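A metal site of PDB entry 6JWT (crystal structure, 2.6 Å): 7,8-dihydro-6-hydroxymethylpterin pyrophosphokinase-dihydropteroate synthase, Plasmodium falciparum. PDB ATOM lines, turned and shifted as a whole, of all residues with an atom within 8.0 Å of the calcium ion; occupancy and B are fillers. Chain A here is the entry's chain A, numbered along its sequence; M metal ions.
The calcium ion is bound by O of Glu 42 (2.5 Å), OE2 of Glu 99 (2.5 Å), O of Gly 46 (2.5 Å), OE1 of Glu 42 (2.6 Å) and OE1 of Glu 99 (2.7 Å).
The backbone NH (N) of Ile 48 sits at hydrogen-bond distance from the side-chain carboxylate (OE2) of Glu 42 (3.1 Å).
The side-chain amino group of Lys 518 is in salt-bridge range of the side-chain carboxylate of Glu 42 (3.7 Å).
The backbone NH (N) of Gly 46 sits at hydrogen-bond distance from the backbone carbonyl oxygen (O) of Val 41 (3.5 Å).
The backbone carbonyl oxygen of Lys 47 is in hydrogen-bond range of the backbone NH of Lys 171 (2.9 Å).
Merely in contact with the calcium ion: Lys 47 (3.9 Å).
The nearest printed residue that does not touch the calcium ion is Glu 98 (4.6 Å).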
ATOM      1  N   HIS A  39      25.930  -4.776 -21.689  1.00  0.00           N
ATOM      2  CA  HIS A  39      25.548  -3.745 -20.735  1.00  0.00           C
ATOM      3  C   HIS A  39      25.161  -2.472 -21.477  1.00  0.00           C
ATOM      4  O   HIS A  39      24.124  -1.876 -21.223  1.00  0.00           O
ATOM      5  CB  HIS A  39      26.684  -3.479 -19.752  1.00  0.00           C
ATOM      6  CG  HIS A  39      26.844  -4.487 -18.661  1.00  0.00           C
ATOM      7  ND1 HIS A  39      28.053  -5.120 -18.407  1.00  0.00           N
ATOM      8  CD2 HIS A  39      25.963  -4.960 -17.742  1.00  0.00           C
ATOM      9  CE1 HIS A  39      27.927  -5.945 -17.393  1.00  0.00           C
ATOM     10  NE2 HIS A  39      26.648  -5.858 -16.963  1.00  0.00           N
ATOM     11  N   LEU A  40      26.018  -2.088 -22.430  1.00  0.00           N
ATOM     12  CA  LEU A  40      25.758  -0.916 -23.253  1.00  0.00           C
ATOM     13  C   LEU A  40      24.527  -1.118 -24.152  1.00  0.00           C
ATOM     14  O   LEU A  40      23.902  -0.134 -24.528  1.00  0.00           O
ATOM     15  CB  LEU A  40      27.009  -0.552 -24.055  1.00  0.00           C
ATOM     16  CG  LEU A  40      28.247  -0.220 -23.207  1.00  0.00           C
ATOM     17  CD1 LEU A  40      29.491  -0.026 -24.064  1.00  0.00           C
ATOM     18  CD2 LEU A  40      28.007   0.965 -22.285  1.00  0.00           C
ATOM     19  N   VAL A  41      24.150  -2.365 -24.452  1.00  0.00           N
ATOM     20  CA  VAL A  41      22.892  -2.579 -25.155  1.00  0.00           C
ATOM     21  C   VAL A  41      21.702  -2.318 -24.234  1.00  0.00           C
ATOM     22  O   VAL A  41      20.701  -1.766 -24.693  1.00  0.00           O
ATOM     23  CB  VAL A  41      22.783  -3.967 -25.819  1.00  0.00           C
ATOM     24  CG1 VAL A  41      21.408  -4.166 -26.446  1.00  0.00           C
ATOM     25  CG2 VAL A  41      23.873  -4.183 -26.853  1.00  0.00           C
ATOM     26  N   GLU A  42      21.797  -2.739 -22.955  1.00  0.00           N
ATOM     27  CA  GLU A  42      20.678  -2.594 -22.021  1.00  0.00           C
ATOM     28  C   GLU A  42      20.506  -1.127 -21.640  1.00  0.00           C
ATOM     29  O   GLU A  42      19.411  -0.677 -21.314  1.00  0.00           O
ATOM     30  CB  GLU A  42      20.867  -3.433 -20.757  1.00  0.00           C
ATOM     31  CG  GLU A  42      20.053  -4.716 -20.742  1.00  0.00           C
ATOM     32  CD  GLU A  42      18.607  -4.667 -20.265  1.00  0.00           C
ATOM     33  OE1 GLU A  42      18.024  -3.551 -20.180  1.00  0.00           O
ATOM     34  OE2 GLU A  42      18.042  -5.774 -19.992  1.00  0.00           O
ATOM     35  N   LYS A  43      21.641  -0.409 -21.675  1.00  0.00           N
ATOM     36  CA  LYS A  43      21.653   0.984 -21.269  1.00  0.00           C
ATOM     37  C   LYS A  43      21.073   1.843 -22.389  1.00  0.00           C
ATOM     38  O   LYS A  43      20.246   2.713 -22.114  1.00  0.00           O
ATOM     39  CB  LYS A  43      23.089   1.399 -20.941  1.00  0.00           C
ATOM     40  CG  LYS A  43      23.288   2.838 -20.478  1.00  0.00           C
ATOM     41  CD  LYS A  43      24.675   3.023 -19.881  1.00  0.00           C
ATOM     42  CE  LYS A  43      24.791   4.170 -18.891  1.00  0.00           C
ATOM     43  NZ  LYS A  43      23.498   4.509 -18.225  1.00  0.00           N
ATOM     44  N   TYR A  44      21.460   1.540 -23.638  1.00  0.00           N
ATOM     45  CA  TYR A  44      21.351   2.467 -24.739  1.00  0.00           C
ATOM     46  C   TYR A  44      20.259   2.075 -25.740  1.00  0.00           C
ATOM     47  O   TYR A  44      19.894   2.900 -26.557  1.00  0.00           O
ATOM     48  CB  TYR A  44      22.708   2.669 -25.431  1.00  0.00           C
ATOM     49  CG  TYR A  44      23.693   3.564 -24.703  1.00  0.00           C
ATOM     50  CD1 TYR A  44      23.269   4.688 -24.007  1.00  0.00           C
ATOM     51  CD2 TYR A  44      25.053   3.312 -24.746  1.00  0.00           C
ATOM     52  CE1 TYR A  44      24.162   5.516 -23.339  1.00  0.00           C
ATOM     53  CE2 TYR A  44      25.957   4.122 -24.085  1.00  0.00           C
ATOM     54  CZ  TYR A  44      25.518   5.233 -23.380  1.00  0.00           C
ATOM     55  OH  TYR A  44      26.416   6.044 -22.727  1.00  0.00           O
ATOM     56  N   LEU A  45      19.717   0.863 -25.685  1.00  0.00           N
ATOM     57  CA  LEU A  45      18.851   0.426 -26.771  1.00  0.00           C
ATOM     58  C   LEU A  45      17.488  -0.054 -26.279  1.00  0.00           C
ATOM     59  O   LEU A  45      16.486   0.045 -26.990  1.00  0.00           O
ATOM     60  CB  LEU A  45      19.542  -0.659 -27.590  1.00  0.00           C
ATOM     61  CG  LEU A  45      20.810  -0.214 -28.319  1.00  0.00           C
ATOM     62  CD1 LEU A  45      21.479  -1.379 -29.053  1.00  0.00           C
ATOM     63  CD2 LEU A  45      20.492   0.918 -29.296  1.00  0.00           C
ATOM     64  N   GLY A  46      17.440  -0.598 -25.063  1.00  0.00           N
ATOM     65  CA  GLY A  46      16.196  -1.134 -24.541  1.00  0.00           C
ATOM     66  C   GLY A  46      16.479  -2.248 -23.553  1.00  0.00           C
ATOM     67  O   GLY A  46      17.508  -2.213 -22.847  1.00  0.00           O
ATOM     68  N   LYS A  47      15.585  -3.252 -23.556  1.00  0.00           N
ATOM     69  CA  LYS A  47      15.633  -4.385 -22.643  1.00  0.00           C
ATOM     70  C   LYS A  47      16.071  -5.657 -23.361  1.00  0.00           C
ATOM     71  O   LYS A  47      15.462  -6.049 -24.363  1.00  0.00           O
ATOM     72  CB  LYS A  47      14.239  -4.542 -22.011  1.00  0.00           C
ATOM     73  CG  LYS A  47      14.213  -5.533 -20.871  1.00  0.00           C
ATOM     74  CD  LYS A  47      12.882  -5.780 -20.220  1.00  0.00           C
ATOM     75  CE  LYS A  47      13.014  -5.861 -18.713  1.00  0.00           C
ATOM     76  NZ  LYS A  47      13.811  -7.040 -18.281  1.00  0.00           N
ATOM     77  N   ILE A  48      17.084  -6.365 -22.839  1.00  0.00           N
ATOM     78  CA  ILE A  48      17.432  -7.706 -23.297  1.00  0.00           C
ATOM     79  C   ILE A  48      16.370  -8.683 -22.776  1.00  0.00           C
ATOM     80  O   ILE A  48      16.167  -8.768 -21.576  1.00  0.00           O
ATOM     81  CB  ILE A  48      18.839  -8.117 -22.825  1.00  0.00           C
ATOM     82  CG1 ILE A  48      19.933  -7.213 -23.391  1.00  0.00           C
ATOM     83  CG2 ILE A  48      19.131  -9.591 -23.117  1.00  0.00           C
ATOM     84  CD1 ILE A  48      21.326  -7.588 -22.933  1.00  0.00           C
ATOM     85  N   SER A  95      21.785   7.551 -20.599  1.00  0.00           N
ATOM     86  CA  SER A  95      20.735   7.390 -21.590  1.00  0.00           C
ATOM     87  C   SER A  95      19.651   8.403 -21.290  1.00  0.00           C
ATOM     88  O   SER A  95      19.535   8.817 -20.144  1.00  0.00           O
ATOM     89  CB  SER A  95      20.139   5.996 -21.548  1.00  0.00           C
ATOM     90  OG  SER A  95      18.940   5.923 -22.336  1.00  0.00           O
ATOM     91  N   TYR A  97      16.624   7.334 -21.873  1.00  0.00           N
ATOM     92  CA  TYR A  97      15.485   6.433 -21.730  1.00  0.00           C
ATOM     93  C   TYR A  97      15.617   5.689 -20.417  1.00  0.00           C
ATOM     94  O   TYR A  97      16.718   5.449 -19.937  1.00  0.00           O
ATOM     95  CB  TYR A  97      15.387   5.481 -22.921  1.00  0.00           C
ATOM     96  CG  TYR A  97      14.644   6.056 -24.104  1.00  0.00           C
ATOM     97  CD1 TYR A  97      15.300   6.913 -24.971  1.00  0.00           C
ATOM     98  CD2 TYR A  97      13.304   5.774 -24.326  1.00  0.00           C
ATOM     99  CE1 TYR A  97      14.642   7.479 -26.054  1.00  0.00           C
ATOM    100  CE2 TYR A  97      12.627   6.340 -25.398  1.00  0.00           C
ATOM    101  CZ  TYR A  97      13.304   7.187 -26.266  1.00  0.00           C
ATOM    102  OH  TYR A  97      12.698   7.761 -27.359  1.00  0.00           O
ATOM    103  N   GLU A  98      14.477   5.318 -19.830  1.00  0.00           N
ATOM    104  CA  GLU A  98      14.560   4.786 -18.484  1.00  0.00           C
ATOM    105  C   GLU A  98      14.870   3.295 -18.526  1.00  0.00           C
ATOM    106  O   GLU A  98      14.619   2.620 -19.534  1.00  0.00           O
ATOM    107  CB  GLU A  98      13.300   5.102 -17.684  1.00  0.00           C
ATOM    108  CG  GLU A  98      12.056   4.521 -18.303  1.00  0.00           C
ATOM    109  CD  GLU A  98      10.809   4.823 -17.489  1.00  0.00           C
ATOM    110  OE1 GLU A  98      10.855   5.748 -16.644  1.00  0.00           O
ATOM    111  OE2 GLU A  98       9.810   4.110 -17.707  1.00  0.00           O
ATOM    112  N   GLU A  99      15.444   2.821 -17.412  1.00  0.00           N
ATOM    113  CA  GLU A  99      15.678   1.423 -17.120  1.00  0.00           C
ATOM    114  C   GLU A  99      14.661   0.940 -16.089  1.00  0.00           C
ATOM    115  O   GLU A  99      14.399   1.651 -15.120  1.00  0.00           O
ATOM    116  CB  GLU A  99      17.097   1.298 -16.570  1.00  0.00           C
ATOM    117  CG  GLU A  99      17.551  -0.127 -16.431  1.00  0.00           C
ATOM    118  CD  GLU A  99      17.571  -0.822 -17.768  1.00  0.00           C
ATOM    119  OE1 GLU A  99      18.613  -0.749 -18.449  1.00  0.00           O
ATOM    120  OE2 GLU A  99      16.541  -1.419 -18.144  1.00  0.00           O
ATOM    121  N   ASN A 100      14.103  -0.264 -16.274  1.00  0.00           N
ATOM    122  CA  ASN A 100      13.101  -0.797 -15.360  1.00  0.00           C
ATOM    123  C   ASN A 100      13.376  -2.268 -15.059  1.00  0.00           C
ATOM    124  O   ASN A 100      13.258  -3.110 -15.928  1.00  0.00           O
ATOM    125  CB  ASN A 100      11.688  -0.646 -15.925  1.00  0.00           C
ATOM    126  CG  ASN A 100      11.254   0.806 -16.017  1.00  0.00           C
ATOM    127  OD1 ASN A 100      10.401   1.143 -16.810  1.00  0.00           O
ATOM    128  ND2 ASN A 100      11.806   1.690 -15.202  1.00  0.00           N
ATOM    129  N   LYS A 101      13.695  -2.576 -13.792  1.00  0.00           N
ATOM    130  CA  LYS A 101      14.153  -3.920 -13.477  1.00  0.00           C
ATOM    131  C   LYS A 101      13.020  -4.820 -12.993  1.00  0.00           C
ATOM    132  O   LYS A 101      13.273  -5.967 -12.663  1.00  0.00           O
ATOM    133  CB  LYS A 101      15.326  -3.873 -12.495  1.00  0.00           C
ATOM    134  CG  LYS A 101      16.509  -3.018 -12.940  1.00  0.00           C
ATOM    135  CD  LYS A 101      17.603  -2.791 -11.882  1.00  0.00           C
ATOM    136  CE  LYS A 101      18.625  -1.768 -12.342  1.00  0.00           C
ATOM    137  NZ  LYS A 101      19.783  -1.618 -11.421  1.00  0.00           N
ATOM    138  N   VAL A 170      16.341  -7.723 -28.230  1.00  0.00           N
ATOM    139  CA  VAL A 170      16.130  -6.469 -27.540  1.00  0.00           C
ATOM    140  C   VAL A 170      14.762  -5.937 -27.882  1.00  0.00           C
ATOM    141  O   VAL A 170      14.429  -5.789 -29.058  1.00  0.00           O
ATOM    142  CB  VAL A 170      17.222  -5.429 -27.866  1.00  0.00           C
ATOM    143  CG1 VAL A 170      17.149  -4.251 -26.908  1.00  0.00           C
ATOM    144  CG2 VAL A 170      18.618  -6.030 -27.851  1.00  0.00           C
ATOM    145  N   LYS A 171      13.954  -5.686 -26.838  1.00  0.00           N
ATOM    146  CA  LYS A 171      12.768  -4.870 -26.963  1.00  0.00           C
ATOM    147  C   LYS A 171      13.221  -3.428 -26.900  1.00  0.00           C
ATOM    148  O   LYS A 171      13.553  -2.928 -25.826  1.00  0.00           O
ATOM    149  CB  LYS A 171      11.795  -5.174 -25.829  1.00  0.00           C
ATOM    150  CG  LYS A 171      10.564  -4.281 -25.745  1.00  0.00           C
ATOM    151  CD  LYS A 171       9.827  -4.481 -24.429  1.00  0.00           C
ATOM    152  CE  LYS A 171       8.949  -5.705 -24.384  1.00  0.00           C
ATOM    153  NZ  LYS A 171       8.702  -6.146 -22.992  1.00  0.00           N
ATOM    154  N   PHE A 173      13.486   0.759 -27.768  1.00  0.00           N
ATOM    155  CA  PHE A 173      12.771   2.014 -27.919  1.00  0.00           C
ATOM    156  C   PHE A 173      13.365   2.817 -29.079  1.00  0.00           C
ATOM    157  O   PHE A 173      13.100   4.011 -29.223  1.00  0.00           O
ATOM    158  CB  PHE A 173      12.822   2.815 -26.615  1.00  0.00           C
ATOM    159  CG  PHE A 173      14.202   2.897 -25.992  1.00  0.00           C
ATOM    160  CD1 PHE A 173      15.220   3.638 -26.581  1.00  0.00           C
ATOM    161  CD2 PHE A 173      14.494   2.240 -24.805  1.00  0.00           C
ATOM    162  CE1 PHE A 173      16.490   3.703 -26.030  1.00  0.00           C
ATOM    163  CE2 PHE A 173      15.758   2.302 -24.238  1.00  0.00           C
ATOM    164  CZ  PHE A 173      16.756   3.033 -24.850  1.00  0.00           C
ATOM    165  N   LYS A 518      22.347  -8.790 -11.890  1.00  0.00           N
ATOM    166  CA  LYS A 518      22.869  -7.805 -12.837  1.00  0.00           C
ATOM    167  C   LYS A 518      23.270  -6.534 -12.088  1.00  0.00           C
ATOM    168  O   LYS A 518      22.465  -6.003 -11.330  1.00  0.00           O
ATOM    169  CB  LYS A 518      21.808  -7.407 -13.864  1.00  0.00           C
ATOM    170  CG  LYS A 518      21.050  -8.569 -14.502  1.00  0.00           C
ATOM    171  CD  LYS A 518      19.604  -8.237 -14.795  1.00  0.00           C
ATOM    172  CE  LYS A 518      19.334  -8.042 -16.273  1.00  0.00           C
ATOM    173  NZ  LYS A 518      18.304  -6.992 -16.484  1.00  0.00           N
HETATM  174 CA    CA M   1      17.063  -1.121 -20.593  1.00  0.00          CA
